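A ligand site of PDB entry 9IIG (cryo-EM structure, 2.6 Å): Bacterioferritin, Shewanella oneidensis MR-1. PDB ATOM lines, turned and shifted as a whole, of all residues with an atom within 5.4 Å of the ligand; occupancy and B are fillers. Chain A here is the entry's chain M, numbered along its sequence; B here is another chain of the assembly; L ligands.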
ATOM      1  N   LEU A  19      16.200 -26.157  24.358  1.00  0.00           N
ATOM      2  CA  LEU A  19      16.469 -26.751  23.050  1.00  0.00           C
ATOM      3  C   LEU A  19      15.447 -26.304  22.017  1.00  0.00           C
ATOM      4  O   LEU A  19      15.803 -25.995  20.868  1.00  0.00           O
ATOM      5  CB  LEU A  19      16.487 -28.276  23.160  1.00  0.00           C
ATOM      6  CG  LEU A  19      17.513 -28.892  24.086  1.00  0.00           C
ATOM      7  CD1 LEU A  19      17.468 -30.386  23.995  1.00  0.00           C
ATOM      8  CD2 LEU A  19      18.879 -28.404  23.712  1.00  0.00           C
ATOM      9  N   ILE A  22      16.470 -22.911  21.044  1.00  0.00           N
ATOM     10  CA  ILE A  22      17.587 -22.928  20.099  1.00  0.00           C
ATOM     11  C   ILE A  22      17.086 -23.146  18.687  1.00  0.00           C
ATOM     12  O   ILE A  22      17.444 -22.427  17.755  1.00  0.00           O
ATOM     13  CB  ILE A  22      18.628 -24.008  20.482  1.00  0.00           C
ATOM     14  CG1 ILE A  22      19.335 -23.668  21.791  1.00  0.00           C
ATOM     15  CG2 ILE A  22      19.663 -24.139  19.397  1.00  0.00           C
ATOM     16  CD1 ILE A  22      19.878 -24.878  22.498  1.00  0.00           C
ATOM     17  N   ASN A  23      16.234 -24.156  18.513  1.00  0.00           N
ATOM     18  CA  ASN A  23      15.767 -24.492  17.173  1.00  0.00           C
ATOM     19  C   ASN A  23      14.946 -23.351  16.579  1.00  0.00           C
ATOM     20  O   ASN A  23      15.140 -22.983  15.415  1.00  0.00           O
ATOM     21  CB  ASN A  23      14.966 -25.782  17.194  1.00  0.00           C
ATOM     22  CG  ASN A  23      15.812 -26.988  16.938  1.00  0.00           C
ATOM     23  OD1 ASN A  23      17.021 -26.880  16.815  1.00  0.00           O
ATOM     24  ND2 ASN A  23      15.186 -28.131  16.804  1.00  0.00           N
ATOM     25  N   PHE A  26      17.150 -20.335  15.681  1.00  0.00           N
ATOM     26  CA  PHE A  26      17.989 -20.519  14.500  1.00  0.00           C
ATOM     27  C   PHE A  26      17.161 -20.503  13.229  1.00  0.00           C
ATOM     28  O   PHE A  26      17.571 -19.897  12.226  1.00  0.00           O
ATOM     29  CB  PHE A  26      18.799 -21.803  14.588  1.00  0.00           C
ATOM     30  CG  PHE A  26      20.081 -21.733  13.832  1.00  0.00           C
ATOM     31  CD1 PHE A  26      21.181 -21.092  14.360  1.00  0.00           C
ATOM     32  CD2 PHE A  26      20.164 -22.234  12.551  1.00  0.00           C
ATOM     33  CE1 PHE A  26      22.356 -21.007  13.648  1.00  0.00           C
ATOM     34  CE2 PHE A  26      21.325 -22.147  11.837  1.00  0.00           C
ATOM     35  CZ  PHE A  26      22.426 -21.523  12.389  1.00  0.00           C
ATOM     36  N   ARG A  30      17.696 -17.651  10.277  1.00  0.00           N
ATOM     37  CA  ARG A  30      17.997 -17.959   8.887  1.00  0.00           C
ATOM     38  C   ARG A  30      16.859 -17.534   7.958  1.00  0.00           C
ATOM     39  O   ARG A  30      17.120 -17.194   6.799  1.00  0.00           O
ATOM     40  CB  ARG A  30      18.343 -19.441   8.772  1.00  0.00           C
ATOM     41  CG  ARG A  30      19.624 -19.709   9.530  1.00  0.00           C
ATOM     42  CD  ARG A  30      20.741 -19.028   8.800  1.00  0.00           C
ATOM     43  NE  ARG A  30      22.062 -19.237   9.373  1.00  0.00           N
ATOM     44  CZ  ARG A  30      22.629 -18.425  10.257  1.00  0.00           C
ATOM     45  NH1 ARG A  30      22.029 -17.308  10.648  1.00  0.00           N
ATOM     46  NH2 ARG A  30      23.822 -18.715  10.739  1.00  0.00           N
ATOM     47  N   TYR A  45      20.575 -15.049  15.858  1.00  0.00           N
ATOM     48  CA  TYR A  45      21.663 -16.014  15.910  1.00  0.00           C
ATOM     49  C   TYR A  45      22.418 -15.940  17.224  1.00  0.00           C
ATOM     50  O   TYR A  45      22.719 -16.976  17.819  1.00  0.00           O
ATOM     51  CB  TYR A  45      22.599 -15.792  14.723  1.00  0.00           C
ATOM     52  CG  TYR A  45      23.824 -16.658  14.750  1.00  0.00           C
ATOM     53  CD1 TYR A  45      23.800 -17.963  14.298  1.00  0.00           C
ATOM     54  CD2 TYR A  45      25.030 -16.154  15.209  1.00  0.00           C
ATOM     55  CE1 TYR A  45      24.920 -18.747  14.334  1.00  0.00           C
ATOM     56  CE2 TYR A  45      26.153 -16.924  15.242  1.00  0.00           C
ATOM     57  CZ  TYR A  45      26.098 -18.220  14.805  1.00  0.00           C
ATOM     58  OH  TYR A  45      27.223 -18.993  14.829  1.00  0.00           O
ATOM     59  N   ILE A  49      22.712 -18.891  19.998  1.00  0.00           N
ATOM     60  CA  ILE A  49      23.974 -19.261  20.631  1.00  0.00           C
ATOM     61  C   ILE A  49      23.865 -19.157  22.144  1.00  0.00           C
ATOM     62  O   ILE A  49      24.431 -19.974  22.890  1.00  0.00           O
ATOM     63  CB  ILE A  49      25.115 -18.379  20.087  1.00  0.00           C
ATOM     64  CG1 ILE A  49      25.242 -18.544  18.580  1.00  0.00           C
ATOM     65  CG2 ILE A  49      26.414 -18.675  20.791  1.00  0.00           C
ATOM     66  CD1 ILE A  49      25.740 -19.867  18.159  1.00  0.00           C
ATOM     67  N   MET A  52      21.979 -21.917  23.429  1.00  0.00           N
ATOM     68  CA  MET A  52      22.895 -23.026  23.285  1.00  0.00           C
ATOM     69  C   MET A  52      23.772 -23.185  24.512  1.00  0.00           C
ATOM     70  O   MET A  52      23.918 -24.281  25.058  1.00  0.00           O
ATOM     71  CB  MET A  52      23.706 -22.748  22.037  1.00  0.00           C
ATOM     72  CG  MET A  52      23.144 -23.332  20.792  1.00  0.00           C
ATOM     73  SD  MET A  52      24.217 -22.837  19.457  1.00  0.00           S
ATOM     74  CE  MET A  52      23.043 -22.243  18.268  1.00  0.00           C
ATOM     75  N   LYS A  53      24.373 -22.084  24.962  1.00  0.00           N
ATOM     76  CA  LYS A  53      25.139 -22.098  26.214  1.00  0.00           C
ATOM     77  C   LYS A  53      24.261 -22.476  27.414  1.00  0.00           C
ATOM     78  O   LYS A  53      24.709 -23.187  28.316  1.00  0.00           O
ATOM     79  CB  LYS A  53      25.785 -20.734  26.446  1.00  0.00           C
ATOM     80  CG  LYS A  53      26.864 -20.377  25.453  1.00  0.00           C
ATOM     81  CD  LYS A  53      27.462 -19.027  25.785  1.00  0.00           C
ATOM     82  CE  LYS A  53      28.615 -18.706  24.873  1.00  0.00           C
ATOM     83  NZ  LYS A  53      28.167 -18.506  23.476  1.00  0.00           N
ATOM     84  N   ALA A  55      21.564 -24.433  27.376  1.00  0.00           N
ATOM     85  CA  ALA A  55      21.317 -25.860  27.305  1.00  0.00           C
ATOM     86  C   ALA A  55      22.549 -26.636  27.716  1.00  0.00           C
ATOM     87  O   ALA A  55      22.445 -27.681  28.373  1.00  0.00           O
ATOM     88  CB  ALA A  55      20.872 -26.249  25.907  1.00  0.00           C
ATOM     89  N   ASP A  56      23.726 -26.154  27.338  1.00  0.00           N
ATOM     90  CA  ASP A  56      24.973 -26.790  27.761  1.00  0.00           C
ATOM     91  C   ASP A  56      25.082 -26.810  29.279  1.00  0.00           C
ATOM     92  O   ASP A  56      25.396 -27.849  29.876  1.00  0.00           O
ATOM     93  CB  ASP A  56      26.149 -26.050  27.129  1.00  0.00           C
ATOM     94  CG  ASP A  56      27.477 -26.648  27.492  1.00  0.00           C
ATOM     95  OD1 ASP A  56      27.529 -27.844  27.811  1.00  0.00           O
ATOM     96  OD2 ASP A  56      28.486 -25.910  27.458  1.00  0.00           O
ATOM     97  N   ILE A  59      22.550 -29.293  30.747  1.00  0.00           N
ATOM     98  CA  ILE A  59      23.006 -30.671  30.561  1.00  0.00           C
ATOM     99  C   ILE A  59      24.096 -31.008  31.556  1.00  0.00           C
ATOM    100  O   ILE A  59      24.081 -32.078  32.179  1.00  0.00           O
ATOM    101  CB  ILE A  59      23.482 -30.902  29.115  1.00  0.00           C
ATOM    102  CG1 ILE A  59      22.334 -30.729  28.128  1.00  0.00           C
ATOM    103  CG2 ILE A  59      24.097 -32.262  28.956  1.00  0.00           C
ATOM    104  CD1 ILE A  59      22.776 -30.394  26.715  1.00  0.00           C
ATOM    105  N   LEU A  71      17.719 -34.795  25.760  1.00  0.00           N
ATOM    106  CA  LEU A  71      17.861 -34.016  24.538  1.00  0.00           C
ATOM    107  C   LEU A  71      16.969 -34.522  23.428  1.00  0.00           C
ATOM    108  O   LEU A  71      17.010 -33.964  22.325  1.00  0.00           O
ATOM    109  CB  LEU A  71      19.315 -34.013  24.068  1.00  0.00           C
ATOM    110  CG  LEU A  71      20.288 -33.074  24.780  1.00  0.00           C
ATOM    111  CD1 LEU A  71      20.625 -33.554  26.174  1.00  0.00           C
ATOM    112  CD2 LEU A  71      21.550 -32.872  23.971  1.00  0.00           C
ATOM    113  N   LEU B  19      20.397 -32.804  12.741  1.00  0.00           N
ATOM    114  CA  LEU B  19      19.988 -32.305  14.052  1.00  0.00           C
ATOM    115  C   LEU B  19      20.042 -33.393  15.102  1.00  0.00           C
ATOM    116  O   LEU B  19      20.497 -33.169  16.238  1.00  0.00           O
ATOM    117  CB  LEU B  19      18.579 -31.722  13.972  1.00  0.00           C
ATOM    118  CG  LEU B  19      18.369 -30.546  13.026  1.00  0.00           C
ATOM    119  CD1 LEU B  19      16.974 -30.029  13.148  1.00  0.00           C
ATOM    120  CD2 LEU B  19      19.343 -29.462  13.365  1.00  0.00           C
ATOM    121  N   ILE B  22      23.595 -33.714  15.996  1.00  0.00           N
ATOM    122  CA  ILE B  22      24.026 -32.650  16.898  1.00  0.00           C
ATOM    123  C   ILE B  22      23.678 -33.015  18.330  1.00  0.00           C
ATOM    124  O   ILE B  22      24.502 -32.931  19.247  1.00  0.00           O
ATOM    125  CB  ILE B  22      23.416 -31.297  16.511  1.00  0.00           C
ATOM    126  CG1 ILE B  22      23.959 -30.789  15.186  1.00  0.00           C
ATOM    127  CG2 ILE B  22      23.699 -30.260  17.574  1.00  0.00           C
ATOM    128  CD1 ILE B  22      23.015 -29.843  14.485  1.00  0.00           C
ATOM    129  N   ASN B  23      22.424 -33.425  18.546  1.00  0.00           N
ATOM    130  CA  ASN B  23      21.979 -33.704  19.905  1.00  0.00           C
ATOM    131  C   ASN B  23      22.741 -34.882  20.510  1.00  0.00           C
ATOM    132  O   ASN B  23      23.197 -34.819  21.652  1.00  0.00           O
ATOM    133  CB  ASN B  23      20.476 -33.970  19.932  1.00  0.00           C
ATOM    134  CG  ASN B  23      19.691 -32.711  20.184  1.00  0.00           C
ATOM    135  OD1 ASN B  23      20.248 -31.628  20.281  1.00  0.00           O
ATOM    136  ND2 ASN B  23      18.393 -32.864  20.357  1.00  0.00           N
ATOM    137  N   PHE B  26      26.391 -33.953  21.289  1.00  0.00           N
ATOM    138  CA  PHE B  26      26.563 -33.087  22.450  1.00  0.00           C
ATOM    139  C   PHE B  26      26.306 -33.835  23.743  1.00  0.00           C
ATOM    140  O   PHE B  26      27.039 -33.669  24.722  1.00  0.00           O
ATOM    141  CB  PHE B  26      25.680 -31.856  22.354  1.00  0.00           C
ATOM    142  CG  PHE B  26      26.252 -30.686  23.085  1.00  0.00           C
ATOM    143  CD1 PHE B  26      27.235 -29.910  22.512  1.00  0.00           C
ATOM    144  CD2 PHE B  26      25.842 -30.398  24.371  1.00  0.00           C
ATOM    145  CE1 PHE B  26      27.775 -28.853  23.192  1.00  0.00           C
ATOM    146  CE2 PHE B  26      26.382 -29.341  25.051  1.00  0.00           C
ATOM    147  CZ  PHE B  26      27.352 -28.565  24.466  1.00  0.00           C
ATOM    148  N   TYR B  45      32.560 -32.774  20.919  1.00  0.00           N
ATOM    149  CA  TYR B  45      32.080 -31.405  20.855  1.00  0.00           C
ATOM    150  C   TYR B  45      32.393 -30.757  19.520  1.00  0.00           C
ATOM    151  O   TYR B  45      31.525 -30.095  18.945  1.00  0.00           O
ATOM    152  CB  TYR B  45      32.671 -30.601  22.013  1.00  0.00           C
ATOM    153  CG  TYR B  45      32.326 -29.144  21.968  1.00  0.00           C
ATOM    154  CD1 TYR B  45      31.116 -28.674  22.446  1.00  0.00           C
ATOM    155  CD2 TYR B  45      33.234 -28.222  21.466  1.00  0.00           C
ATOM    156  CE1 TYR B  45      30.816 -27.336  22.403  1.00  0.00           C
ATOM    157  CE2 TYR B  45      32.939 -26.892  21.426  1.00  0.00           C
ATOM    158  CZ  TYR B  45      31.727 -26.453  21.890  1.00  0.00           C
ATOM    159  OH  TYR B  45      31.435 -25.109  21.847  1.00  0.00           O
ATOM    160  N   ILE B  49      29.698 -29.430  16.795  1.00  0.00           N
ATOM    161  CA  ILE B  49      29.808 -28.127  16.143  1.00  0.00           C
ATOM    162  C   ILE B  49      29.828 -28.295  14.622  1.00  0.00           C
ATOM    163  O   ILE B  49      29.269 -27.470  13.886  1.00  0.00           O
ATOM    164  CB  ILE B  49      31.066 -27.398  16.640  1.00  0.00           C
ATOM    165  CG1 ILE B  49      31.005 -27.188  18.146  1.00  0.00           C
ATOM    166  CG2 ILE B  49      31.265 -26.086  15.904  1.00  0.00           C
ATOM    167  CD1 ILE B  49      29.974 -26.219  18.576  1.00  0.00           C
ATOM    168  N   MET B  52      26.527 -29.022  13.440  1.00  0.00           N
ATOM    169  CA  MET B  52      25.842 -27.752  13.590  1.00  0.00           C
ATOM    170  C   MET B  52      25.994 -26.903  12.332  1.00  0.00           C
ATOM    171  O   MET B  52      25.017 -26.362  11.811  1.00  0.00           O
ATOM    172  CB  MET B  52      26.443 -27.086  14.810  1.00  0.00           C
ATOM    173  CG  MET B  52      25.724 -27.356  16.079  1.00  0.00           C
ATOM    174  SD  MET B  52      26.622 -26.535  17.377  1.00  0.00           S
ATOM    175  CE  MET B  52      26.760 -27.828  18.587  1.00  0.00           C
ATOM    176  N   LYS B  53      27.225 -26.770  11.844  1.00  0.00           N
ATOM    177  CA  LYS B  53      27.467 -26.085  10.584  1.00  0.00           C
ATOM    178  C   LYS B  53      26.759 -26.772   9.416  1.00  0.00           C
ATOM    179  O   LYS B  53      26.240 -26.098   8.512  1.00  0.00           O
ATOM    180  CB  LYS B  53      28.962 -25.992  10.306  1.00  0.00           C
ATOM    181  CG  LYS B  53      29.724 -25.109  11.262  1.00  0.00           C
ATOM    182  CD  LYS B  53      31.196 -25.075  10.890  1.00  0.00           C
ATOM    183  CE  LYS B  53      31.958 -24.105  11.764  1.00  0.00           C
ATOM    184  NZ  LYS B  53      32.005 -24.569  13.168  1.00  0.00           N
ATOM    185  N   ALA B  55      23.933 -28.535   9.555  1.00  0.00           N
ATOM    186  CA  ALA B  55      22.521 -28.224   9.659  1.00  0.00           C
ATOM    187  C   ALA B  55      22.243 -26.790   9.236  1.00  0.00           C
ATOM    188  O   ALA B  55      21.235 -26.508   8.604  1.00  0.00           O
ATOM    189  CB  ALA B  55      22.027 -28.464  11.085  1.00  0.00           C
ATOM    190  N   ASP B  56      23.152 -25.876   9.573  1.00  0.00           N
ATOM    191  CA  ASP B  56      23.021 -24.498   9.130  1.00  0.00           C
ATOM    192  C   ASP B  56      22.997 -24.408   7.608  1.00  0.00           C
ATOM    193  O   ASP B  56      22.139 -23.742   7.023  1.00  0.00           O
ATOM    194  CB  ASP B  56      24.165 -23.670   9.714  1.00  0.00           C
ATOM    195  CG  ASP B  56      24.109 -22.222   9.328  1.00  0.00           C
ATOM    196  OD1 ASP B  56      22.999 -21.729   9.028  1.00  0.00           O
ATOM    197  OD2 ASP B  56      25.158 -21.559   9.326  1.00  0.00           O
ATOM    198  N   ILE B  59      19.709 -25.847   6.258  1.00  0.00           N
ATOM    199  CA  ILE B  59      18.604 -24.902   6.456  1.00  0.00           C
ATOM    200  C   ILE B  59      18.675 -23.785   5.427  1.00  0.00           C
ATOM    201  O   ILE B  59      17.667 -23.413   4.837  1.00  0.00           O
ATOM    202  CB  ILE B  59      18.620 -24.346   7.893  1.00  0.00           C
ATOM    203  CG1 ILE B  59      18.363 -25.459   8.907  1.00  0.00           C
ATOM    204  CG2 ILE B  59      17.588 -23.261   8.059  1.00  0.00           C
ATOM    205  CD1 ILE B  59      18.885 -25.148  10.291  1.00  0.00           C
ATOM    206  N   LEU B  71      12.932 -28.171  11.469  1.00  0.00           N
ATOM    207  CA  LEU B  71      13.740 -28.301  12.660  1.00  0.00           C
ATOM    208  C   LEU B  71      12.967 -28.922  13.815  1.00  0.00           C
ATOM    209  O   LEU B  71      13.520 -29.072  14.904  1.00  0.00           O
ATOM    210  CB  LEU B  71      14.304 -26.952  13.102  1.00  0.00           C
ATOM    211  CG  LEU B  71      15.519 -26.413  12.344  1.00  0.00           C
ATOM    212  CD1 LEU B  71      15.157 -25.950  10.951  1.00  0.00           C
ATOM    213  CD2 LEU B  71      16.203 -25.316  13.117  1.00  0.00           C
HETATM  214  C1  LIG L   1      27.901 -23.353  18.149  1.00  0.00           C
HETATM  215  C2  LIG L   1      25.592 -25.845  21.674  1.00  0.00           C
HETATM  216  C3  LIG L   1      22.204 -27.062  18.390  1.00  0.00           C
HETATM  217  C4  LIG L   1      24.170 -24.082  15.091  1.00  0.00           C
HETATM  218  C5  LIG L   1      27.573 -23.876  19.392  1.00  0.00           C
HETATM  219  C6  LIG L   1      28.250 -23.636  20.647  1.00  0.00           C
HETATM  220  C7  LIG L   1      27.628 -24.324  21.620  1.00  0.00           C
HETATM  221  C8  LIG L   1      26.508 -25.027  21.021  1.00  0.00           C
HETATM  222  C9  LIG L   1      28.009 -24.352  23.114  1.00  0.00           C
HETATM  223  C10 LIG L   1      29.503 -22.736  20.785  1.00  0.00           C
HETATM  224  C11 LIG L   1      29.076 -21.356  21.233  1.00  0.00           C
HETATM  225  C12 LIG L   1      30.282 -20.489  21.486  1.00  0.00           C
HETATM  226  O1  LIG L   1      30.298 -19.344  20.980  1.00  0.00           O
HETATM  227  O2  LIG L   1      31.227 -20.923  22.174  1.00  0.00           O
HETATM  228  C13 LIG L   1      24.483 -26.422  21.090  1.00  0.00           C
HETATM  229  C14 LIG L   1      23.522 -27.299  21.730  1.00  0.00           C
HETATM  230  C15 LIG L   1      22.585 -27.625  20.811  1.00  0.00           C
HETATM  231  C16 LIG L   1      22.911 -26.976  19.570  1.00  0.00           C
HETATM  232  C17 LIG L   1      23.607 -27.728  23.202  1.00  0.00           C
HETATM  233  C18 LIG L   1      21.362 -28.560  20.974  1.00  0.00           C
HETATM  234  C19 LIG L   1      21.351 -29.595  21.817  1.00  0.00           C
HETATM  235  C20 LIG L   1      22.417 -26.352  17.234  1.00  0.00           C
HETATM  236  C21 LIG L   1      21.588 -26.386  16.046  1.00  0.00           C
HETATM  237  C22 LIG L   1      22.120 -25.565  15.135  1.00  0.00           C
HETATM  238  C23 LIG L   1      23.321 -24.980  15.699  1.00  0.00           C
HETATM  239  C24 LIG L   1      20.308 -27.245  15.937  1.00  0.00           C
HETATM  240  C25 LIG L   1      21.659 -25.223  13.694  1.00  0.00           C
HETATM  241  C26 LIG L   1      20.590 -25.718  13.085  1.00  0.00           C
HETATM  242  C27 LIG L   1      25.380 -23.671  15.603  1.00  0.00           C
HETATM  243  C28 LIG L   1      26.391 -22.905  14.901  1.00  0.00           C
HETATM  244  C29 LIG L   1      27.413 -22.722  15.739  1.00  0.00           C
HETATM  245  C30 LIG L   1      27.110 -23.334  17.006  1.00  0.00           C
HETATM  246  C31 LIG L   1      26.274 -22.430  13.445  1.00  0.00           C
HETATM  247  C32 LIG L   1      28.708 -21.952  15.416  1.00  0.00           C
HETATM  248  C33 LIG L   1      29.859 -22.913  15.145  1.00  0.00           C
HETATM  249  C34 LIG L   1      31.027 -22.518  16.016  1.00  0.00           C
HETATM  250  O3  LIG L   1      30.908 -22.603  17.271  1.00  0.00           O
HETATM  251  O4  LIG L   1      32.075 -22.120  15.455  1.00  0.00           O
HETATM  252  N1  LIG L   1      26.512 -24.724  19.671  1.00  0.00           N
HETATM  253  N2  LIG L   1      24.072 -26.256  19.778  1.00  0.00           N
HETATM  254  N3  LIG L   1      23.455 -25.486  16.979  1.00  0.00           N
HETATM  255  N4  LIG L   1      25.850 -23.906  16.886  1.00  0.00           N
HETATM  256 FE1  LIG L   1      24.913 -25.163  18.298  1.00  0.00          FE
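Leu 19 of chain A touches the ligand (CD2 to C19, 3.3 Å).
Asn 23 of chain A touches the ligand.
CD2 of Phe 26 of chain A touches C25 of the ligand, 3.5 Å away.
Tyr 45 of chain A touches the ligand.
Ile 49 of chain A touches the ligand (CG2 to C11, 3.8 Å).
CD2 of Leu 71 of chain A touches C19 of the ligand, 3.9 Å away.
Leu 19 of chain B touches the ligand (CD2 to C24, 3.5 Å).
Ile 22 of chain B touches the ligand (CG2 to C3, 3.6 Å).
OD1 of Asn 23 of chain B touches C19 of the ligand (2.8 Å).
Phe 26 of chain B touches the ligand.
OH of Tyr 45 of chain B touches C10 of the ligand, 3.2 Å away.
Ile 49 of chain B touches the ligand.
CB of Ala 55 of chain B touches C26 of the ligand, at 3.7 Å.
Ile 59 of chain B touches the ligand (CD1 to C26, 3.3 Å).
Hydrophobic or aromatic side chains that line the ligand: Leu 19 of chain A, Phe 26 of chain A, Ile 49 of chain A, Met 52 of chain A, Leu 71 of chain A, Leu 19 of chain B, Ile 22 of chain B, Phe 26 of chain B, Ile 49 of chain B, Met 52 of chain B, Ala 55 of chain B and Ile 59 of chain B.
Within 4 Å of the ligand: Leu 19 of chain A, Asn 23 of chain A, Phe 26 of chain A, Tyr 45 of chain A, Ile 49 of chain A, Met 52 of chain A, Lys 53 of chain A, Leu 71 of chain A, Leu 19 of chain B, Ile 22 of chain B, Asn 23 of chain B, Phe 26 of chain B, Tyr 45 of chain B, Ile 49 of chain B, Met 52 of chain B, Lys 53 of chain B, Ala 55 of chain B and Ile 59 of chain B.
The side-chain amide nitrogen of Asn 23 of chain A is in hydrogen-bond range of the backbone carbonyl oxygen of Leu 71 of chain B (2.7 Å).
The side-chain amide nitrogen (ND2) of Asn 23 of chain B lies within hydrogen-bond range of the backbone carbonyl oxygen (O) of Leu 71 of chain A (2.6 Å).
FE1 of the ligand is bound by SD of Met 52 of chain A (2.7 Å).
The side-chain amino group (NZ) of Lys 53 of chain B lies within salt-bridge range of an oxygen (O4) of the ligand (3.4 Å).
FE1 of the ligand is bound by SD of Met 52 of chain B.
The side-chain amino group (NZ) of Lys 53 of chain A is in salt-bridge range of an oxygen (O1) of the ligand, 3.4 Å away.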
